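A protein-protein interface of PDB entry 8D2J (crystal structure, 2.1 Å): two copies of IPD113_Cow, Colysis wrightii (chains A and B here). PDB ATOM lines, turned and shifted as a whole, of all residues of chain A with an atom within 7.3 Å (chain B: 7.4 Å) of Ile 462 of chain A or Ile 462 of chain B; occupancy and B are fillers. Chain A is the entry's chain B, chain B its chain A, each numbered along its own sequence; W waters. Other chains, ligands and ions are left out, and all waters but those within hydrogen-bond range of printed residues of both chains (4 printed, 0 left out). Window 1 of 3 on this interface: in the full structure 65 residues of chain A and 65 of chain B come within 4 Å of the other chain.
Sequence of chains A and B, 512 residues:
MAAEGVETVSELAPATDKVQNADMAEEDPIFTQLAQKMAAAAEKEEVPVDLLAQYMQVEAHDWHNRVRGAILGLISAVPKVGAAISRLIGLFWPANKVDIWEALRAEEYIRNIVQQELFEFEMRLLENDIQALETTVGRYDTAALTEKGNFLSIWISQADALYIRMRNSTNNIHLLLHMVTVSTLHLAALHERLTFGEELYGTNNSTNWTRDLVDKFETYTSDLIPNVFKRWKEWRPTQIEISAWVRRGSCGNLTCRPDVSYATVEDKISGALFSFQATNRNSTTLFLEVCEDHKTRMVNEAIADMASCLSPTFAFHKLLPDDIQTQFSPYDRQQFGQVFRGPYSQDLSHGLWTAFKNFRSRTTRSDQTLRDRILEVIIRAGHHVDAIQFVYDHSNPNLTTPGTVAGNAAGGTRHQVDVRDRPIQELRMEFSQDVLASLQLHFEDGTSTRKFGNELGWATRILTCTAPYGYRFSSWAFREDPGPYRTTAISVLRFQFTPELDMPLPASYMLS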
ATOM      1  N   SER A 349      26.060 -12.254  32.834  1.00  0.00           N
ATOM      2  CA  SER A 349      26.018 -10.773  32.681  1.00  0.00           C
ATOM      3  C   SER A 349      24.870 -10.156  33.491  1.00  0.00           C
ATOM      4  O   SER A 349      24.942  -8.939  33.758  1.00  0.00           O
ATOM      5  CB  SER A 349      25.906 -10.376  31.236  1.00  0.00           C
ATOM      6  OG  SER A 349      26.863 -11.059  30.448  1.00  0.00           O
ATOM      7  N   ARG A 428      35.225  -9.996  20.698  1.00  0.00           N
ATOM      8  CA  ARG A 428      33.897  -9.429  21.056  1.00  0.00           C
ATOM      9  C   ARG A 428      32.828 -10.502  20.845  1.00  0.00           C
ATOM     10  O   ARG A 428      32.791 -11.094  19.753  1.00  0.00           O
ATOM     11  CB  ARG A 428      33.576  -8.179  20.234  1.00  0.00           C
ATOM     12  CG  ARG A 428      32.303  -7.467  20.670  1.00  0.00           C
ATOM     13  CD  ARG A 428      32.380  -5.970  20.429  1.00  0.00           C
ATOM     14  NE  ARG A 428      33.232  -5.299  21.404  1.00  0.00           N
ATOM     15  CZ  ARG A 428      33.852  -4.135  21.209  1.00  0.00           C
ATOM     16  NH1 ARG A 428      33.743  -3.497  20.055  1.00  0.00           N
ATOM     17  NH2 ARG A 428      34.594  -3.619  22.172  1.00  0.00           N
ATOM     18  N   MET A 429      31.994 -10.724  21.861  1.00  0.00           N
ATOM     19  CA  MET A 429      30.898 -11.726  21.864  1.00  0.00           C
ATOM     20  C   MET A 429      29.567 -10.995  22.041  1.00  0.00           C
ATOM     21  O   MET A 429      29.469 -10.163  22.961  1.00  0.00           O
ATOM     22  CB  MET A 429      31.076 -12.723  23.014  1.00  0.00           C
ATOM     23  CG  MET A 429      32.328 -13.567  22.903  1.00  0.00           C
ATOM     24  SD  MET A 429      32.912 -14.131  24.521  1.00  0.00           S
ATOM     25  CE  MET A 429      33.717 -12.643  25.109  1.00  0.00           C
ATOM     26  N   GLU A 430      28.591 -11.282  21.177  1.00  0.00           N
ATOM     27  CA  GLU A 430      27.177 -10.874  21.365  1.00  0.00           C
ATOM     28  C   GLU A 430      26.389 -12.121  21.766  1.00  0.00           C
ATOM     29  O   GLU A 430      26.540 -13.150  21.087  1.00  0.00           O
ATOM     30  CB  GLU A 430      26.610 -10.234  20.098  1.00  0.00           C
ATOM     31  CG  GLU A 430      27.295  -8.933  19.718  1.00  0.00           C
ATOM     32  CD  GLU A 430      26.703  -8.237  18.505  1.00  0.00           C
ATOM     33  OE1 GLU A 430      26.169  -8.937  17.623  1.00  0.00           O
ATOM     34  OE2 GLU A 430      26.769  -6.995  18.447  1.00  0.00           O
ATOM     35  N   PHE A 431      25.609 -12.031  22.845  1.00  0.00           N
ATOM     36  CA  PHE A 431      24.700 -13.104  23.322  1.00  0.00           C
ATOM     37  C   PHE A 431      23.255 -12.674  23.063  1.00  0.00           C
ATOM     38  O   PHE A 431      22.903 -11.525  23.386  1.00  0.00           O
ATOM     39  CB  PHE A 431      24.944 -13.405  24.801  1.00  0.00           C
ATOM     40  CG  PHE A 431      26.305 -13.978  25.103  1.00  0.00           C
ATOM     41  CD1 PHE A 431      26.523 -15.346  25.049  1.00  0.00           C
ATOM     42  CD2 PHE A 431      27.364 -13.151  25.443  1.00  0.00           C
ATOM     43  CE1 PHE A 431      27.775 -15.873  25.323  1.00  0.00           C
ATOM     44  CE2 PHE A 431      28.616 -13.681  25.718  1.00  0.00           C
ATOM     45  CZ  PHE A 431      28.818 -15.041  25.658  1.00  0.00           C
ATOM     46  N   SER A 438      27.150 -13.747  17.909  1.00  0.00           N
ATOM     47  CA  SER A 438      28.225 -13.311  16.981  1.00  0.00           C
ATOM     48  C   SER A 438      29.584 -13.297  17.681  1.00  0.00           C
ATOM     49  O   SER A 438      29.623 -13.203  18.925  1.00  0.00           O
ATOM     50  CB  SER A 438      27.902 -11.967  16.377  1.00  0.00           C
ATOM     51  OG  SER A 438      28.089 -10.923  17.317  1.00  0.00           O
ATOM     52  N   GLN A 440      33.679 -11.466  16.883  1.00  0.00           N
ATOM     53  CA  GLN A 440      34.520 -10.517  16.102  1.00  0.00           C
ATOM     54  C   GLN A 440      35.927 -10.511  16.707  1.00  0.00           C
ATOM     55  O   GLN A 440      36.030 -10.551  17.949  1.00  0.00           O
ATOM     56  CB  GLN A 440      33.898  -9.118  16.100  1.00  0.00           C
ATOM     57  CG  GLN A 440      34.573  -8.143  15.142  1.00  0.00           C
ATOM     58  CD  GLN A 440      33.859  -6.816  15.046  1.00  0.00           C
ATOM     59  OE1 GLN A 440      33.061  -6.449  15.908  1.00  0.00           O
ATOM     60  NE2 GLN A 440      34.148  -6.074  13.990  1.00  0.00           N
ATOM     61  N   ASN A 454      24.717 -12.616  13.619  1.00  0.00           N
ATOM     62  CA  ASN A 454      23.836 -11.512  14.092  1.00  0.00           C
ATOM     63  C   ASN A 454      24.047 -10.264  13.222  1.00  0.00           C
ATOM     64  O   ASN A 454      24.122  -9.157  13.786  1.00  0.00           O
ATOM     65  CB  ASN A 454      24.081 -11.205  15.573  1.00  0.00           C
ATOM     66  CG  ASN A 454      23.034 -10.285  16.164  1.00  0.00           C
ATOM     67  OD1 ASN A 454      21.854 -10.405  15.848  1.00  0.00           O
ATOM     68  ND2 ASN A 454      23.454  -9.363  17.014  1.00  0.00           N
ATOM     69  N   TRP A 458      19.455  -7.599  17.006  1.00  0.00           N
ATOM     70  CA  TRP A 458      19.730  -6.810  18.235  1.00  0.00           C
ATOM     71  C   TRP A 458      20.410  -7.715  19.267  1.00  0.00           C
ATOM     72  O   TRP A 458      19.827  -8.764  19.591  1.00  0.00           O
ATOM     73  CB  TRP A 458      18.433  -6.208  18.786  1.00  0.00           C
ATOM     74  CG  TRP A 458      18.631  -5.382  20.019  1.00  0.00           C
ATOM     75  CD1 TRP A 458      18.607  -5.812  21.315  1.00  0.00           C
ATOM     76  CD2 TRP A 458      18.907  -3.972  20.068  1.00  0.00           C
ATOM     77  NE1 TRP A 458      18.842  -4.767  22.167  1.00  0.00           N
ATOM     78  CE2 TRP A 458      19.026  -3.625  21.432  1.00  0.00           C
ATOM     79  CE3 TRP A 458      19.057  -2.973  19.100  1.00  0.00           C
ATOM     80  CZ2 TRP A 458      19.292  -2.320  21.844  1.00  0.00           C
ATOM     81  CZ3 TRP A 458      19.319  -1.684  19.509  1.00  0.00           C
ATOM     82  CH2 TRP A 458      19.436  -1.366  20.863  1.00  0.00           C
ATOM     83  N   ALA A 459      21.589  -7.323  19.755  1.00  0.00           N
ATOM     84  CA  ALA A 459      22.361  -8.059  20.783  1.00  0.00           C
ATOM     85  C   ALA A 459      21.756  -7.778  22.162  1.00  0.00           C
ATOM     86  O   ALA A 459      21.633  -6.598  22.522  1.00  0.00           O
ATOM     87  CB  ALA A 459      23.815  -7.662  20.728  1.00  0.00           C
ATOM     88  N   THR A 460      21.380  -8.825  22.900  1.00  0.00           N
ATOM     89  CA  THR A 460      20.904  -8.714  24.303  1.00  0.00           C
ATOM     90  C   THR A 460      22.081  -8.281  25.179  1.00  0.00           C
ATOM     91  O   THR A 460      21.922  -7.306  25.933  1.00  0.00           O
ATOM     92  CB  THR A 460      20.273 -10.021  24.795  1.00  0.00           C
ATOM     93  OG1 THR A 460      19.178 -10.320  23.930  1.00  0.00           O
ATOM     94  CG2 THR A 460      19.796  -9.938  26.230  1.00  0.00           C
ATOM     95  N   ARG A 461      23.211  -8.985  25.065  1.00  0.00           N
ATOM     96  CA  ARG A 461      24.471  -8.702  25.802  1.00  0.00           C
ATOM     97  C   ARG A 461      25.634  -8.616  24.811  1.00  0.00           C
ATOM     98  O   ARG A 461      25.651  -9.410  23.848  1.00  0.00           O
ATOM     99  CB  ARG A 461      24.737  -9.790  26.846  1.00  0.00           C
ATOM    100  CG  ARG A 461      23.831  -9.714  28.065  1.00  0.00           C
ATOM    101  CD  ARG A 461      24.163  -8.525  28.944  1.00  0.00           C
ATOM    102  NE  ARG A 461      23.183  -8.343  30.005  1.00  0.00           N
ATOM    103  CZ  ARG A 461      23.271  -7.444  30.978  1.00  0.00           C
ATOM    104  NH1 ARG A 461      24.312  -6.629  31.050  1.00  0.00           N
ATOM    105  NH2 ARG A 461      22.314  -7.367  31.886  1.00  0.00           N
ATOM    106  N   ILE A 462      26.549  -7.671  25.045  1.00  0.00           N
ATOM    107  CA  ILE A 462      27.831  -7.502  24.297  1.00  0.00           C
ATOM    108  C   ILE A 462      28.971  -7.535  25.319  1.00  0.00           C
ATOM    109  O   ILE A 462      28.943  -6.714  26.254  1.00  0.00           O
ATOM    110  CB  ILE A 462      27.840  -6.196  23.478  1.00  0.00           C
ATOM    111  CG1 ILE A 462      26.570  -6.043  22.634  1.00  0.00           C
ATOM    112  CG2 ILE A 462      29.100  -6.114  22.628  1.00  0.00           C
ATOM    113  CD1 ILE A 462      26.400  -4.674  22.015  1.00  0.00           C
ATOM    114  N   LEU A 463      29.919  -8.460  25.147  1.00  0.00           N
ATOM    115  CA  LEU A 463      31.089  -8.647  26.047  1.00  0.00           C
ATOM    116  C   LEU A 463      32.369  -8.641  25.212  1.00  0.00           C
ATOM    117  O   LEU A 463      32.358  -9.216  24.112  1.00  0.00           O
ATOM    118  CB  LEU A 463      30.929  -9.967  26.805  1.00  0.00           C
ATOM    119  CG  LEU A 463      29.965  -9.908  27.986  1.00  0.00           C
ATOM    120  CD1 LEU A 463      29.195 -11.210  28.127  1.00  0.00           C
ATOM    121  CD2 LEU A 463      30.704  -9.567  29.272  1.00  0.00           C
ATOM    122  N   THR A 464      33.420  -8.002  25.728  1.00  0.00           N
ATOM    123  CA  THR A 464      34.769  -7.947  25.111  1.00  0.00           C
ATOM    124  C   THR A 464      35.739  -8.707  26.020  1.00  0.00           C
ATOM    125  O   THR A 464      35.810  -8.372  27.214  1.00  0.00           O
ATOM    126  CB  THR A 464      35.190  -6.495  24.854  1.00  0.00           C
ATOM    127  OG1 THR A 464      34.189  -5.903  24.026  1.00  0.00           O
ATOM    128  CG2 THR A 464      36.544  -6.378  24.188  1.00  0.00           C
ATOM    129  N   SER B 349      32.899   8.082  27.933  1.00  0.00           N
ATOM    130  CA  SER B 349      32.963   6.643  28.311  1.00  0.00           C
ATOM    131  C   SER B 349      34.290   6.308  29.005  1.00  0.00           C
ATOM    132  O   SER B 349      34.315   5.305  29.748  1.00  0.00           O
ATOM    133  CB  SER B 349      32.733   5.760  27.114  1.00  0.00           C
ATOM    134  OG  SER B 349      31.363   5.777  26.742  1.00  0.00           O
ATOM    135  N   ARG B 428      20.936   2.071  20.313  1.00  0.00           N
ATOM    136  CA  ARG B 428      22.338   1.610  20.480  1.00  0.00           C
ATOM    137  C   ARG B 428      23.248   2.460  19.593  1.00  0.00           C
ATOM    138  O   ARG B 428      22.998   2.518  18.374  1.00  0.00           O
ATOM    139  CB  ARG B 428      22.487   0.128  20.135  1.00  0.00           C
ATOM    140  CG  ARG B 428      23.864  -0.439  20.447  1.00  0.00           C
ATOM    141  CD  ARG B 428      23.771  -1.929  20.710  1.00  0.00           C
ATOM    142  NE  ARG B 428      23.223  -2.184  22.039  1.00  0.00           N
ATOM    143  CZ  ARG B 428      22.606  -3.299  22.419  1.00  0.00           C
ATOM    144  NH1 ARG B 428      22.421  -4.293  21.566  1.00  0.00           N
ATOM    145  NH2 ARG B 428      22.164  -3.409  23.661  1.00  0.00           N
ATOM    146  N   MET B 429      24.254   3.089  20.204  1.00  0.00           N
ATOM    147  CA  MET B 429      25.266   3.942  19.533  1.00  0.00           C
ATOM    148  C   MET B 429      26.631   3.258  19.635  1.00  0.00           C
ATOM    149  O   MET B 429      27.006   2.844  20.747  1.00  0.00           O
ATOM    150  CB  MET B 429      25.355   5.313  20.209  1.00  0.00           C
ATOM    151  CG  MET B 429      24.077   6.123  20.129  1.00  0.00           C
ATOM    152  SD  MET B 429      23.889   7.217  21.555  1.00  0.00           S
ATOM    153  CE  MET B 429      23.421   6.023  22.808  1.00  0.00           C
ATOM    154  N   GLU B 430      27.341   3.149  18.514  1.00  0.00           N
ATOM    155  CA  GLU B 430      28.777   2.779  18.480  1.00  0.00           C
ATOM    156  C   GLU B 430      29.586   4.039  18.174  1.00  0.00           C
ATOM    157  O   GLU B 430      29.186   4.787  17.258  1.00  0.00           O
ATOM    158  CB  GLU B 430      29.048   1.708  17.425  1.00  0.00           C
ATOM    159  CG  GLU B 430      28.292   0.417  17.668  1.00  0.00           C
ATOM    160  CD  GLU B 430      28.587  -0.668  16.650  1.00  0.00           C
ATOM    161  OE1 GLU B 430      28.802  -0.323  15.469  1.00  0.00           O
ATOM    162  OE2 GLU B 430      28.603  -1.852  17.040  1.00  0.00           O
ATOM    163  N   PHE B 431      30.669   4.263  18.921  1.00  0.00           N
ATOM    164  CA  PHE B 431      31.637   5.361  18.679  1.00  0.00           C
ATOM    165  C   PHE B 431      32.947   4.748  18.179  1.00  0.00           C
ATOM    166  O   PHE B 431      33.380   3.707  18.720  1.00  0.00           O
ATOM    167  CB  PHE B 431      31.802   6.220  19.936  1.00  0.00           C
ATOM    168  CG  PHE B 431      30.546   6.943  20.349  1.00  0.00           C
ATOM    169  CD1 PHE B 431      30.282   8.227  19.892  1.00  0.00           C
ATOM    170  CD2 PHE B 431      29.616   6.335  21.180  1.00  0.00           C
ATOM    171  CE1 PHE B 431      29.120   8.887  20.263  1.00  0.00           C
ATOM    172  CE2 PHE B 431      28.458   7.000  21.553  1.00  0.00           C
ATOM    173  CZ  PHE B 431      28.210   8.274  21.093  1.00  0.00           C
ATOM    174  N   SER B 438      27.778   4.159  14.255  1.00  0.00           N
ATOM    175  CA  SER B 438      26.507   3.485  13.894  1.00  0.00           C
ATOM    176  C   SER B 438      25.386   3.846  14.872  1.00  0.00           C
ATOM    177  O   SER B 438      25.686   4.302  15.997  1.00  0.00           O
ATOM    178  CB  SER B 438      26.699   1.995  13.822  1.00  0.00           C
ATOM    179  OG  SER B 438      26.903   1.450  15.114  1.00  0.00           O
ATOM    180  N   GLN B 440      21.343   1.985  15.922  1.00  0.00           N
ATOM    181  CA  GLN B 440      20.365   0.873  15.769  1.00  0.00           C
ATOM    182  C   GLN B 440      19.190   1.124  16.720  1.00  0.00           C
ATOM    183  O   GLN B 440      19.443   1.476  17.883  1.00  0.00           O
ATOM    184  CB  GLN B 440      21.043  -0.472  16.047  1.00  0.00           C
ATOM    185  CG  GLN B 440      20.161  -1.680  15.758  1.00  0.00           C
ATOM    186  CD  GLN B 440      20.835  -2.992  16.083  1.00  0.00           C
ATOM    187  OE1 GLN B 440      21.794  -3.049  16.849  1.00  0.00           O
ATOM    188  NE2 GLN B 440      20.329  -4.068  15.505  1.00  0.00           N
ATOM    189  N   ASN B 454      29.104   1.523  10.189  1.00  0.00           N
ATOM    190  CA  ASN B 454      30.137   0.638  10.795  1.00  0.00           C
ATOM    191  C   ASN B 454      29.796  -0.829  10.496  1.00  0.00           C
ATOM    192  O   ASN B 454      29.812  -1.650  11.439  1.00  0.00           O
ATOM    193  CB  ASN B 454      30.270   0.894  12.302  1.00  0.00           C
ATOM    194  CG  ASN B 454      31.498   0.250  12.914  1.00  0.00           C
ATOM    195  OD1 ASN B 454      32.538   0.146  12.268  1.00  0.00           O
ATOM    196  ND2 ASN B 454      31.388  -0.191  14.158  1.00  0.00           N
ATOM    197  N   TRP B 458      35.348  -2.148  13.689  1.00  0.00           N
ATOM    198  CA  TRP B 458      35.379  -2.430  15.148  1.00  0.00           C
ATOM    199  C   TRP B 458      34.896  -1.190  15.905  1.00  0.00           C
ATOM    200  O   TRP B 458      35.427  -0.093  15.642  1.00  0.00           O
ATOM    201  CB  TRP B 458      36.793  -2.841  15.576  1.00  0.00           C
ATOM    202  CG  TRP B 458      36.940  -3.103  17.043  1.00  0.00           C
ATOM    203  CD1 TRP B 458      37.262  -2.198  18.011  1.00  0.00           C
ATOM    204  CD2 TRP B 458      36.763  -4.363  17.713  1.00  0.00           C
ATOM    205  NE1 TRP B 458      37.297  -2.808  19.236  1.00  0.00           N
ATOM    206  CE2 TRP B 458      36.997  -4.135  19.085  1.00  0.00           C
ATOM    207  CE3 TRP B 458      36.438  -5.657  17.291  1.00  0.00           C
ATOM    208  CZ2 TRP B 458      36.913  -5.153  20.033  1.00  0.00           C
ATOM    209  CZ3 TRP B 458      36.355  -6.663  18.228  1.00  0.00           C
ATOM    210  CH2 TRP B 458      36.591  -6.411  19.581  1.00  0.00           C
ATOM    211  N   ALA B 459      33.920  -1.359  16.800  1.00  0.00           N
ATOM    212  CA  ALA B 459      33.390  -0.284  17.672  1.00  0.00           C
ATOM    213  C   ALA B 459      34.332  -0.108  18.867  1.00  0.00           C
ATOM    214  O   ALA B 459      34.573  -1.106  19.573  1.00  0.00           O
ATOM    215  CB  ALA B 459      31.985  -0.618  18.115  1.00  0.00           C
ATOM    216  N   THR B 460      34.854   1.108  19.068  1.00  0.00           N
ATOM    217  CA  THR B 460      35.677   1.488  20.248  1.00  0.00           C
ATOM    218  C   THR B 460      34.790   1.474  21.497  1.00  0.00           C
ATOM    219  O   THR B 460      35.238   0.937  22.530  1.00  0.00           O
ATOM    220  CB  THR B 460      36.340   2.858  20.063  1.00  0.00           C
ATOM    221  OG1 THR B 460      37.159   2.806  18.895  1.00  0.00           O
ATOM    222  CG2 THR B 460      37.177   3.275  21.254  1.00  0.00           C
ATOM    223  N   ARG B 461      33.593   2.062  21.399  1.00  0.00           N
ATOM    224  CA  ARG B 461      32.590   2.120  22.496  1.00  0.00           C
ATOM    225  C   ARG B 461      31.208   1.760  21.950  1.00  0.00           C
ATOM    226  O   ARG B 461      30.889   2.155  20.806  1.00  0.00           O
ATOM    227  CB  ARG B 461      32.556   3.509  23.141  1.00  0.00           C
ATOM    228  CG  ARG B 461      33.798   3.851  23.945  1.00  0.00           C
ATOM    229  CD  ARG B 461      33.948   2.976  25.176  1.00  0.00           C
ATOM    230  NE  ARG B 461      35.090   3.378  25.981  1.00  0.00           N
ATOM    231  CZ  ARG B 461      35.411   2.863  27.165  1.00  0.00           C
ATOM    232  NH1 ARG B 461      34.676   1.907  27.710  1.00  0.00           N
ATOM    233  NH2 ARG B 461      36.475   3.314  27.804  1.00  0.00           N
ATOM    234  N   ILE B 462      30.438   1.017  22.745  1.00  0.00           N
ATOM    235  CA  ILE B 462      29.018   0.662  22.470  1.00  0.00           C
ATOM    236  C   ILE B 462      28.188   1.123  23.671  1.00  0.00           C
ATOM    237  O   ILE B 462      28.454   0.646  24.793  1.00  0.00           O
ATOM    238  CB  ILE B 462      28.861  -0.847  22.196  1.00  0.00           C
ATOM    239  CG1 ILE B 462      29.825  -1.328  21.106  1.00  0.00           C
ATOM    240  CG2 ILE B 462      27.412  -1.174  21.857  1.00  0.00           C
ATOM    241  CD1 ILE B 462      29.887  -2.828  20.950  1.00  0.00           C
ATOM    242  N   LEU B 463      27.229   2.020  23.435  1.00  0.00           N
ATOM    243  CA  LEU B 463      26.345   2.593  24.483  1.00  0.00           C
ATOM    244  C   LEU B 463      24.882   2.365  24.095  1.00  0.00           C
ATOM    245  O   LEU B 463      24.548   2.500  22.897  1.00  0.00           O
ATOM    246  CB  LEU B 463      26.679   4.078  24.638  1.00  0.00           C
ATOM    247  CG  LEU B 463      28.034   4.353  25.287  1.00  0.00           C
ATOM    248  CD1 LEU B 463      28.754   5.493  24.590  1.00  0.00           C
ATOM    249  CD2 LEU B 463      27.884   4.628  26.775  1.00  0.00           C
ATOM    250  N   THR B 464      24.056   1.995  25.075  1.00  0.00           N
ATOM    251  CA  THR B 464      22.602   1.750  24.904  1.00  0.00           C
ATOM    252  C   THR B 464      21.838   2.794  25.722  1.00  0.00           C
ATOM    253  O   THR B 464      22.023   2.845  26.957  1.00  0.00           O
ATOM    254  CB  THR B 464      22.234   0.307  25.273  1.00  0.00           C
ATOM    255  OG1 THR B 464      23.122  -0.554  24.563  1.00  0.00           O
ATOM    256  CG2 THR B 464      20.804  -0.047  24.927  1.00  0.00           C
HETATM  257  O   HOH W   1      32.768  -3.931  17.376  1.00  0.00           O
HETATM  258  O   HOH W   2      36.403  -1.499  22.488  1.00  0.00           O
HETATM  259  O   HOH W   3      20.595  -5.174  25.291  1.00  0.00           O
HETATM  260  O   HOH W   4      22.686  -4.716  18.764  1.00  0.00           O
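Water W3 lies within hydrogen-bond range of the backbone carbonyl oxygen of Thr 460 of chain A (2.6 Å), the guanidinium group of Arg 428 of chain B (2.9 Å) and the backbone carbonyl oxygen of Ala 459 of chain A (3.3 Å).
Water W4 lies within hydrogen-bond range of OE1 of Gln 440 of chain B, NH1 of Arg 428 of chain B and N of Ala 459 of chain A.
Water W2 lies within hydrogen-bond range of O of Thr 460 of chain B, NH2 of Arg 428 of chain A and O of Ala 459 of chain B.
Water W1 lies within hydrogen-bond range of N of Ala 459 of chain B (2.9 Å), NH1 of Arg 428 of chain A (2.9 Å) and OE1 of Gln 440 of chain A (2.9 Å).
The guanidinium group of Arg 428 of chain B lies within hydrogen-bond range of the side-chain hydroxyl of Thr 464 of chain B (3.0 Å).
O of Gln 440 of chain A lies within hydrogen-bond range of N of Arg 428 of chain A.
O of Gln 440 of chain B sits at hydrogen-bond distance from N of Arg 428 of chain B (2.9 Å).
The guanidinium group (NE) of Arg 428 of chain A lies within hydrogen-bond range of the side-chain hydroxyl (OG1) of Thr 464 of chain A (2.9 Å).
The guanidinium group (NH1) of Arg 428 of chain A is in hydrogen-bond range of the backbone carbonyl oxygen (O) of Ala 459 of chain B, 2.6 Å away.
The guanidinium group (NH1) of Arg 428 of chain B is in hydrogen-bond range of the backbone carbonyl oxygen (O) of Ala 459 of chain A, at 2.6 Å.
CZ2 of Trp 458 of chain B touches CZ of Arg 428 of chain A (3.4 Å).
Gln 440 of chain A touches Trp 458 of chain B.
Trp 458 of chain A touches Arg 428 of chain B (CE2 to NH1, 3.5 Å).
Trp 458 of chain A touches Gln 440 of chain B (CE3 to CD, 3.5 Å).
CG2 of Ile 462 of chain B touches CD1 of Ile 462 of chain A, at 3.6 Å.
Arg 428 of chain A touches Trp 458 of chain B, and with the chains exchanged Trp 458 of chain A touches Arg 428 of chain B.
Arg 428 of chain A touches Ala 459 of chain B, and with the chains exchanged Ala 459 of chain A touches Arg 428 of chain B.
Gln 440 of chain A touches Trp 458 of chain B, and with the chains exchanged Trp 458 of chain A touches Gln 440 of chain B.
Ile 462 of chain A touches its own counterpart, Ile 462 of chain B.
15 positions are printed for both chains.
Hydrophobic or aromatic side chains of chain A that line the printed part of chain B: Trp 458, Ala 459 and Ile 462.
Hydrophobic or aromatic side chains of chain B that line the printed part of chain A: Trp 458, Ala 459 and Ile 462.
Of the printed residues of chain B, Ile 462 of chain A touches Ile 462.
Of the printed residues of chain A, Ile 462 of chain B touches Ile 462 (3.6 Å).
Of the printed residues of chain B, Ala 459 of chain A touches Arg 428 (2.6 Å).
Of the printed residues of chain B, Arg 428 of chain A touches Trp 458 (3.4 Å) and Ala 459 (2.6 Å).
The nearest printed residue of chain A that does not touch Ile 462 of chain B is Arg 428 of chain A (4.01 Å).
The nearest printed residue of chain A that does not touch Trp 458 of chain B is Thr 464 of chain A (4.3 Å).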
